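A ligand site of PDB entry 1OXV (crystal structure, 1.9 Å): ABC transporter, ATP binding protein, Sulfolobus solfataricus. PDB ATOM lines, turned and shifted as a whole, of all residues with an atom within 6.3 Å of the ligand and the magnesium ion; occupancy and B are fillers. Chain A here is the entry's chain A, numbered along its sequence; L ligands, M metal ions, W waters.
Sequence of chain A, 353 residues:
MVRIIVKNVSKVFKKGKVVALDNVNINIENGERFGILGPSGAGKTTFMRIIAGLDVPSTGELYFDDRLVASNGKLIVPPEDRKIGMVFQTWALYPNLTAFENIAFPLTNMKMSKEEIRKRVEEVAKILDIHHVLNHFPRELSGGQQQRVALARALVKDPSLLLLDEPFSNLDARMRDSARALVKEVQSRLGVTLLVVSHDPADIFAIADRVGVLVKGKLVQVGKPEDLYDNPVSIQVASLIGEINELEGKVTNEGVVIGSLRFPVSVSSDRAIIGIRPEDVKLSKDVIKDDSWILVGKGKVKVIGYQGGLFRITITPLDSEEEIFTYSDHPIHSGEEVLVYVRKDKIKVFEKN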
ATOM      1  N   PHE A  13       1.215  -6.331 -15.611  1.00  0.00           N
ATOM      2  CA  PHE A  13       1.784  -6.544 -16.936  1.00  0.00           C
ATOM      3  C   PHE A  13       0.670  -6.296 -17.963  1.00  0.00           C
ATOM      4  O   PHE A  13      -0.489  -6.101 -17.592  1.00  0.00           O
ATOM      5  CB  PHE A  13       2.317  -7.978 -17.084  1.00  0.00           C
ATOM      6  CG  PHE A  13       3.513  -8.285 -16.204  1.00  0.00           C
ATOM      7  CD1 PHE A  13       3.414  -9.204 -15.167  1.00  0.00           C
ATOM      8  CD2 PHE A  13       4.720  -7.625 -16.393  1.00  0.00           C
ATOM      9  CE1 PHE A  13       4.517  -9.495 -14.340  1.00  0.00           C
ATOM     10  CE2 PHE A  13       5.815  -7.889 -15.580  1.00  0.00           C
ATOM     11  CZ  PHE A  13       5.723  -8.820 -14.542  1.00  0.00           C
ATOM     12  N   LYS A  14       1.009  -6.341 -19.233  1.00  0.00           N
ATOM     13  CA  LYS A  14       0.036  -6.140 -20.307  1.00  0.00           C
ATOM     14  C   LYS A  14      -0.735  -4.842 -20.132  1.00  0.00           C
ATOM     15  O   LYS A  14      -1.957  -4.783 -20.261  1.00  0.00           O
ATOM     16  CB  LYS A  14      -0.923  -7.335 -20.424  1.00  0.00           C
ATOM     17  CG  LYS A  14      -0.297  -8.558 -21.096  1.00  0.00           C
ATOM     18  CD  LYS A  14      -1.337  -9.667 -21.307  1.00  0.00           C
ATOM     19  CE  LYS A  14      -0.856 -10.736 -22.280  1.00  0.00           C
ATOM     20  NZ  LYS A  14       0.438 -11.339 -21.865  1.00  0.00           N
ATOM     21  N   VAL A  18      -3.117  -7.629 -16.680  1.00  0.00           N
ATOM     22  CA  VAL A  18      -2.722  -8.761 -15.855  1.00  0.00           C
ATOM     23  C   VAL A  18      -2.136  -8.264 -14.538  1.00  0.00           C
ATOM     24  O   VAL A  18      -1.155  -7.535 -14.529  1.00  0.00           O
ATOM     25  CB  VAL A  18      -1.678  -9.614 -16.587  1.00  0.00           C
ATOM     26  CG1 VAL A  18      -1.029 -10.621 -15.636  1.00  0.00           C
ATOM     27  CG2 VAL A  18      -2.295 -10.298 -17.781  1.00  0.00           C
ATOM     28  N   VAL A  19      -2.762  -8.630 -13.430  1.00  0.00           N
ATOM     29  CA  VAL A  19      -2.268  -8.224 -12.120  1.00  0.00           C
ATOM     30  C   VAL A  19      -1.519  -9.402 -11.536  1.00  0.00           C
ATOM     31  O   VAL A  19      -2.131 -10.348 -11.013  1.00  0.00           O
ATOM     32  CB  VAL A  19      -3.414  -7.739 -11.209  1.00  0.00           C
ATOM     33  CG1 VAL A  19      -2.911  -7.378  -9.830  1.00  0.00           C
ATOM     34  CG2 VAL A  19      -4.124  -6.561 -11.855  1.00  0.00           C
ATOM     35  N   ALA A  20      -0.206  -9.344 -11.658  1.00  0.00           N
ATOM     36  CA  ALA A  20       0.670 -10.456 -11.250  1.00  0.00           C
ATOM     37  C   ALA A  20       0.787 -10.536  -9.726  1.00  0.00           C
ATOM     38  O   ALA A  20       0.938 -11.619  -9.150  1.00  0.00           O
ATOM     39  CB  ALA A  20       2.037 -10.309 -11.896  1.00  0.00           C
ATOM     40  N   GLY A  38       2.878 -21.587  -3.981  1.00  0.00           N
ATOM     41  CA  GLY A  38       1.750 -21.190  -4.791  1.00  0.00           C
ATOM     42  C   GLY A  38       1.800 -21.887  -6.118  1.00  0.00           C
ATOM     43  O   GLY A  38       2.853 -22.298  -6.575  1.00  0.00           O
ATOM     44  N   PRO A  39       0.640 -22.015  -6.737  1.00  0.00           N
ATOM     45  CA  PRO A  39       0.509 -22.687  -8.039  1.00  0.00           C
ATOM     46  C   PRO A  39       1.259 -21.957  -9.149  1.00  0.00           C
ATOM     47  O   PRO A  39       1.637 -20.791  -9.014  1.00  0.00           O
ATOM     48  CB  PRO A  39      -0.995 -22.594  -8.323  1.00  0.00           C
ATOM     49  CG  PRO A  39      -1.651 -22.257  -7.051  1.00  0.00           C
ATOM     50  CD  PRO A  39      -0.650 -21.512  -6.235  1.00  0.00           C
ATOM     51  N   SER A  40       1.471 -22.650 -10.254  1.00  0.00           N
ATOM     52  CA  SER A  40       2.098 -22.029 -11.406  1.00  0.00           C
ATOM     53  C   SER A  40       1.285 -20.777 -11.750  1.00  0.00           C
ATOM     54  O   SER A  40       0.053 -20.813 -11.760  1.00  0.00           O
ATOM     55  CB  SER A  40       2.115 -22.989 -12.590  1.00  0.00           C
ATOM     56  OG  SER A  40       2.678 -22.376 -13.732  1.00  0.00           O
ATOM     57  N   GLY A  41       1.972 -19.663 -11.997  1.00  0.00           N
ATOM     58  CA  GLY A  41       1.312 -18.433 -12.390  1.00  0.00           C
ATOM     59  C   GLY A  41       0.847 -17.546 -11.247  1.00  0.00           C
ATOM     60  O   GLY A  41       0.302 -16.477 -11.497  1.00  0.00           O
ATOM     61  N   ALA A  42       1.054 -17.983 -10.013  1.00  0.00           N
ATOM     62  CA  ALA A  42       0.613 -17.215  -8.839  1.00  0.00           C
ATOM     63  C   ALA A  42       1.336 -15.885  -8.630  1.00  0.00           C
ATOM     64  O   ALA A  42       0.804 -14.998  -7.966  1.00  0.00           O
ATOM     65  CB  ALA A  42       0.720 -18.066  -7.586  1.00  0.00           C
ATOM     66  N   GLY A  43       2.538 -15.762  -9.171  1.00  0.00           N
ATOM     67  CA  GLY A  43       3.324 -14.553  -9.028  1.00  0.00           C
ATOM     68  C   GLY A  43       4.623 -14.711  -8.229  1.00  0.00           C
ATOM     69  O   GLY A  43       5.242 -13.720  -7.867  1.00  0.00           O
ATOM     70  N   LYS A  44       5.064 -15.956  -8.035  1.00  0.00           N
ATOM     71  CA  LYS A  44       6.268 -16.234  -7.245  1.00  0.00           C
ATOM     72  C   LYS A  44       7.540 -15.604  -7.805  1.00  0.00           C
ATOM     73  O   LYS A  44       8.250 -14.902  -7.096  1.00  0.00           O
ATOM     74  CB  LYS A  44       6.450 -17.759  -7.080  1.00  0.00           C
ATOM     75  CG  LYS A  44       5.283 -18.423  -6.413  1.00  0.00           C
ATOM     76  CD  LYS A  44       5.465 -19.947  -6.248  1.00  0.00           C
ATOM     77  CE  LYS A  44       5.701 -20.662  -7.576  1.00  0.00           C
ATOM     78  NZ  LYS A  44       4.518 -20.648  -8.501  1.00  0.00           N
ATOM     79  N   THR A  45       7.805 -15.851  -9.087  1.00  0.00           N
ATOM     80  CA  THR A  45       8.994 -15.298  -9.730  1.00  0.00           C
ATOM     81  C   THR A  45       8.909 -13.773  -9.809  1.00  0.00           C
ATOM     82  O   THR A  45       9.902 -13.079  -9.674  1.00  0.00           O
ATOM     83  CB  THR A  45       9.196 -15.916 -11.128  1.00  0.00           C
ATOM     84  OG1 THR A  45       9.594 -17.288 -11.016  1.00  0.00           O
ATOM     85  CG2 THR A  45      10.373 -15.269 -11.845  1.00  0.00           C
ATOM     86  N   THR A  46       7.722 -13.246 -10.061  1.00  0.00           N
ATOM     87  CA  THR A  46       7.565 -11.811 -10.116  1.00  0.00           C
ATOM     88  C   THR A  46       7.956 -11.218  -8.754  1.00  0.00           C
ATOM     89  O   THR A  46       8.692 -10.234  -8.666  1.00  0.00           O
ATOM     90  CB  THR A  46       6.126 -11.456 -10.472  1.00  0.00           C
ATOM     91  OG1 THR A  46       5.812 -11.971 -11.780  1.00  0.00           O
ATOM     92  CG2 THR A  46       5.965  -9.952 -10.569  1.00  0.00           C
ATOM     93  N   PHE A  47       7.483 -11.849  -7.699  1.00  0.00           N
ATOM     94  CA  PHE A  47       7.817 -11.412  -6.358  1.00  0.00           C
ATOM     95  C   PHE A  47       9.316 -11.428  -6.122  1.00  0.00           C
ATOM     96  O   PHE A  47       9.896 -10.441  -5.658  1.00  0.00           O
ATOM     97  CB  PHE A  47       7.098 -12.291  -5.359  1.00  0.00           C
ATOM     98  CG  PHE A  47       7.366 -11.942  -3.948  1.00  0.00           C
ATOM     99  CD1 PHE A  47       6.761 -10.854  -3.354  1.00  0.00           C
ATOM    100  CD2 PHE A  47       8.235 -12.687  -3.211  1.00  0.00           C
ATOM    101  CE1 PHE A  47       7.029 -10.537  -2.056  1.00  0.00           C
ATOM    102  CE2 PHE A  47       8.489 -12.371  -1.914  1.00  0.00           C
ATOM    103  CZ  PHE A  47       7.887 -11.309  -1.335  1.00  0.00           C
ATOM    104  N   ASP A  55      13.138  -6.047 -11.049  1.00  0.00           N
ATOM    105  CA  ASP A  55      11.891  -5.418 -11.453  1.00  0.00           C
ATOM    106  C   ASP A  55      11.490  -4.544 -10.282  1.00  0.00           C
ATOM    107  O   ASP A  55      12.133  -4.606  -9.225  1.00  0.00           O
ATOM    108  CB  ASP A  55      10.819  -6.457 -11.748  1.00  0.00           C
ATOM    109  CG  ASP A  55       9.735  -5.941 -12.685  1.00  0.00           C
ATOM    110  OD1 ASP A  55       9.607  -4.710 -12.870  1.00  0.00           O
ATOM    111  OD2 ASP A  55       8.971  -6.719 -13.296  1.00  0.00           O
ATOM    112  N   GLN A  89      15.192 -19.851 -11.250  1.00  0.00           N
ATOM    113  CA  GLN A  89      14.546 -21.060 -11.735  1.00  0.00           C
ATOM    114  C   GLN A  89      15.292 -21.645 -12.932  1.00  0.00           C
ATOM    115  O   GLN A  89      15.428 -22.857 -13.046  1.00  0.00           O
ATOM    116  CB  GLN A  89      13.080 -20.787 -12.107  1.00  0.00           C
ATOM    117  CG  GLN A  89      12.098 -21.724 -11.397  1.00  0.00           C
ATOM    118  CD  GLN A  89      11.099 -22.348 -12.348  1.00  0.00           C
ATOM    119  OE1 GLN A  89       9.895 -22.098 -12.246  1.00  0.00           O
ATOM    120  NE2 GLN A  89      11.586 -23.179 -13.263  1.00  0.00           N
ATOM    121  N   ASP A 165      14.817 -19.459  -6.415  1.00  0.00           N
ATOM    122  CA  ASP A 165      13.566 -19.640  -7.149  1.00  0.00           C
ATOM    123  C   ASP A 165      13.503 -21.060  -7.715  1.00  0.00           C
ATOM    124  O   ASP A 165      14.134 -21.387  -8.716  1.00  0.00           O
ATOM    125  CB  ASP A 165      13.409 -18.597  -8.256  1.00  0.00           C
ATOM    126  CG  ASP A 165      11.997 -18.539  -8.830  1.00  0.00           C
ATOM    127  OD1 ASP A 165      11.145 -19.373  -8.422  1.00  0.00           O
ATOM    128  OD2 ASP A 165      11.641 -17.687  -9.688  1.00  0.00           O
ATOM    129  N   GLU A 166      12.728 -21.902  -7.047  1.00  0.00           N
ATOM    130  CA  GLU A 166      12.542 -23.290  -7.447  1.00  0.00           C
ATOM    131  C   GLU A 166      13.860 -23.963  -7.750  1.00  0.00           C
ATOM    132  O   GLU A 166      14.093 -24.393  -8.875  1.00  0.00           O
ATOM    133  CB  GLU A 166      11.620 -23.384  -8.663  1.00  0.00           C
ATOM    134  CG  GLU A 166      10.281 -22.679  -8.475  1.00  0.00           C
ATOM    135  CD  GLU A 166       9.165 -23.329  -9.265  1.00  0.00           C
ATOM    136  OE1 GLU A 166       9.161 -24.573  -9.346  1.00  0.00           O
ATOM    137  OE2 GLU A 166       8.290 -22.604  -9.796  1.00  0.00           O
ATOM    138  N   SER A 198       8.632 -22.032  -4.361  1.00  0.00           N
ATOM    139  CA  SER A 198       8.344 -23.323  -4.933  1.00  0.00           C
ATOM    140  C   SER A 198       6.858 -23.578  -5.053  1.00  0.00           C
ATOM    141  O   SER A 198       6.044 -22.994  -4.353  1.00  0.00           O
ATOM    142  CB  SER A 198       8.941 -24.422  -4.068  1.00  0.00           C
ATOM    143  OG  SER A 198       8.498 -25.679  -4.545  1.00  0.00           O
ATOM    144  N   HIS A 199       6.521 -24.489  -5.962  1.00  0.00           N
ATOM    145  CA  HIS A 199       5.161 -24.991  -6.069  1.00  0.00           C
ATOM    146  C   HIS A 199       5.155 -26.353  -5.390  1.00  0.00           C
ATOM    147  O   HIS A 199       4.203 -27.121  -5.521  1.00  0.00           O
ATOM    148  CB  HIS A 199       4.727 -25.116  -7.534  1.00  0.00           C
ATOM    149  CG  HIS A 199       5.646 -25.972  -8.352  1.00  0.00           C
ATOM    150  ND1 HIS A 199       6.365 -25.482  -9.417  1.00  0.00           N
ATOM    151  CD2 HIS A 199       5.954 -27.286  -8.245  1.00  0.00           C
ATOM    152  CE1 HIS A 199       7.086 -26.463  -9.941  1.00  0.00           C
ATOM    153  NE2 HIS A 199       6.858 -27.562  -9.251  1.00  0.00           N
ATOM    154  N   LEU A 214       0.776 -17.849  -2.023  1.00  0.00           N
ATOM    155  CA  LEU A 214       0.403 -16.901  -3.043  1.00  0.00           C
ATOM    156  C   LEU A 214      -0.540 -17.592  -4.012  1.00  0.00           C
ATOM    157  O   LEU A 214      -0.203 -18.650  -4.540  1.00  0.00           O
ATOM    158  CB  LEU A 214       1.687 -16.502  -3.776  1.00  0.00           C
ATOM    159  CG  LEU A 214       1.809 -15.164  -4.460  1.00  0.00           C
ATOM    160  CD1 LEU A 214       1.479 -14.020  -3.517  1.00  0.00           C
ATOM    161  CD2 LEU A 214       3.238 -15.038  -4.997  1.00  0.00           C
HETATM  162  P1  LIG L   1       5.661 -20.757 -12.047  1.00  0.00           P
HETATM  163  O1  LIG L   1       5.333 -21.438 -10.754  1.00  0.00           O
HETATM  164  O2  LIG L   1       5.253 -21.549 -13.256  1.00  0.00           O
HETATM  165  O3  LIG L   1       7.114 -20.533 -12.111  1.00  0.00           O
HETATM  166  P2  LIG L   1       5.095 -18.028 -11.121  1.00  0.00           P
HETATM  167  O4  LIG L   1       4.393 -18.234  -9.841  1.00  0.00           O
HETATM  168  O5  LIG L   1       6.549 -17.845 -10.913  1.00  0.00           O
HETATM  169  N1  LIG L   1       4.816 -19.328 -12.127  1.00  0.00           N
HETATM  170  P3  LIG L   1       5.078 -15.600 -12.527  1.00  0.00           P
HETATM  171  O6  LIG L   1       5.439 -14.617 -11.461  1.00  0.00           O
HETATM  172  O7  LIG L   1       6.240 -15.876 -13.383  1.00  0.00           O
HETATM  173  O8  LIG L   1       4.415 -16.831 -11.854  1.00  0.00           O
HETATM  174  O9  LIG L   1       4.056 -14.913 -13.409  1.00  0.00           O
HETATM  175  C1  LIG L   1       2.928 -14.366 -12.777  1.00  0.00           C
HETATM  176  C2  LIG L   1       1.897 -13.850 -13.793  1.00  0.00           C
HETATM  177  O10 LIG L   1       2.428 -12.728 -14.460  1.00  0.00           O
HETATM  178  C3  LIG L   1       1.572 -14.809 -14.923  1.00  0.00           C
HETATM  179  O11 LIG L   1       0.245 -14.547 -15.392  1.00  0.00           O
HETATM  180  C4  LIG L   1       2.568 -14.467 -16.007  1.00  0.00           C
HETATM  181  O12 LIG L   1       2.121 -14.762 -17.315  1.00  0.00           O
HETATM  182  C5  LIG L   1       2.682 -12.969 -15.842  1.00  0.00           C
HETATM  183  N2  LIG L   1       3.990 -12.426 -16.200  1.00  0.00           N
HETATM  184  C6  LIG L   1       5.153 -12.601 -15.532  1.00  0.00           C
HETATM  185  N3  LIG L   1       6.152 -11.910 -16.158  1.00  0.00           N
HETATM  186  C7  LIG L   1       5.610 -11.284 -17.216  1.00  0.00           C
HETATM  187  C8  LIG L   1       6.083 -10.396 -18.297  1.00  0.00           C
HETATM  188  N4  LIG L   1       7.417 -10.014 -18.370  1.00  0.00           N
HETATM  189  N5  LIG L   1       5.184  -9.981 -19.193  1.00  0.00           N
HETATM  190  C9  LIG L   1       3.891 -10.322 -19.151  1.00  0.00           C
HETATM  191  N6  LIG L   1       3.396 -11.139 -18.200  1.00  0.00           N
HETATM  192  C10 LIG L   1       4.184 -11.622 -17.238  1.00  0.00           C
HETATM  193 MG    MG M   1       8.246 -18.903 -11.525  1.00  0.00          MG
HETATM  194  O   HOH W   1      -1.237 -15.727 -13.564  1.00  0.00           O
HETATM  195  O   HOH W   2       0.938 -11.624 -19.008  1.00  0.00           O
HETATM  196  O   HOH W   3       8.580 -19.803  -9.751  1.00  0.00           O
HETATM  197  O   HOH W   4       9.660 -10.399 -16.402  1.00  0.00           O
HETATM  198  O   HOH W   5       7.935 -11.432 -13.694  1.00  0.00           O
HETATM  199  O   HOH W   6       8.209 -14.227 -14.238  1.00  0.00           O
HETATM  200  O   HOH W   7       7.919 -17.924 -13.528  1.00  0.00           O
HETATM  201  O   HOH W   8       3.872 -18.473 -14.824  1.00  0.00           O
HETATM  202  O   HOH W   9      10.018 -19.757 -12.365  1.00  0.00           O
HETATM  203  O   HOH W  10      -2.564 -14.079 -16.836  1.00  0.00           O
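An oxygen (O5) of the ligand lies close to the backbone NH (N) of Thr 45 (3.0 Å).
The backbone NH (N) of Lys 44 is in hydrogen-bond range of an oxygen (O4) of the ligand, 3.0 Å away.
NZ of Lys 44 is in salt-bridge range of O1 of the ligand, at 2.5 Å.
An oxygen (O6) of the ligand sits at hydrogen-bond distance from the backbone NH of Thr 46, at 3.0 Å.
OG1 of Thr 46 is in hydrogen-bond range of O6 of the ligand (2.7 Å).
OG of Ser 40 is in hydrogen-bond range of O2 of the ligand (2.7 Å).
O4 of the ligand lies within hydrogen-bond range of N of Gly 43.
OE1 of Gln 89 lies close to O3 of the ligand (3.2 Å).
An oxygen (O4) of the ligand is in hydrogen-bond range of the backbone NH of Ala 42, at 3.4 Å.
The side-chain hydroxyl (OG1) of Thr 45 lies close to the side-chain carboxylate (OD2) of Asp 165, 2.5 Å away.
NZ of Lys 44 sits at hydrogen-bond distance from O of Pro 39 (2.9 Å).
The backbone carbonyl oxygen (O) of Gly 38 sits at hydrogen-bond distance from the side-chain amino group (NZ) of Lys 44, at 3.0 Å.
The side-chain amide oxygen (OE1) of Gln 89 lies close to the side-chain carboxylate (OE2) of Glu 166 (3.0 Å).
The backbone NH (N) of Gln 89 sits close to the backbone carbonyl oxygen (O) of Asp 165 (3.1 Å).
N of Phe 13 is in hydrogen-bond range of O of Val 18 (2.9 Å).
The side-chain carboxylate of Glu 166 lies close to a ring nitrogen (ND1) of His 199, at 2.9 Å.
The backbone NH of Gly 41 sits close to a nitrogen (N1) of the ligand.
OE2 of Glu 166 sits close to O1 of the ligand.
Merely in contact with the ligand: Phe 13, Ala 20 and Pro 39.
12 residues have an atom within 4 Å of the ligand: Phe 13, Ala 20, Pro 39, Ser 40, Gly 41, Ala 42, Gly 43, Lys 44, Thr 45, Thr 46, Gln 89 and Glu 166.
The nearest printed residue that does not touch the ligand is Val 18 (4.1 Å).
Gln 89 touches the magnesium ion (OE1 to MG, 3.7 Å).
Two residues have an atom within 4 Å of the magnesium ion: Thr 45 and Gln 89.
The magnesium ion is bound by water W3, an oxygen (O3) of the ligand, an oxygen (O5) of the ligand, water W9, the side-chain hydroxyl of Thr 45 and water W7.
The magnesium ion has six donor atoms within binding distance.
Water W3 lies within hydrogen-bond range of OE2 of Glu 166 and OD1 of Asp 165.
Water W2 bridges N6 of the ligand (2.6 Å) and NZ of Lys 14 (2.9 Å).
Water W1 lies within hydrogen-bond range of O11 of the ligand and O of Gly 41.
Water W5 bridges OG1 of Thr 46 and N3 of the ligand.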
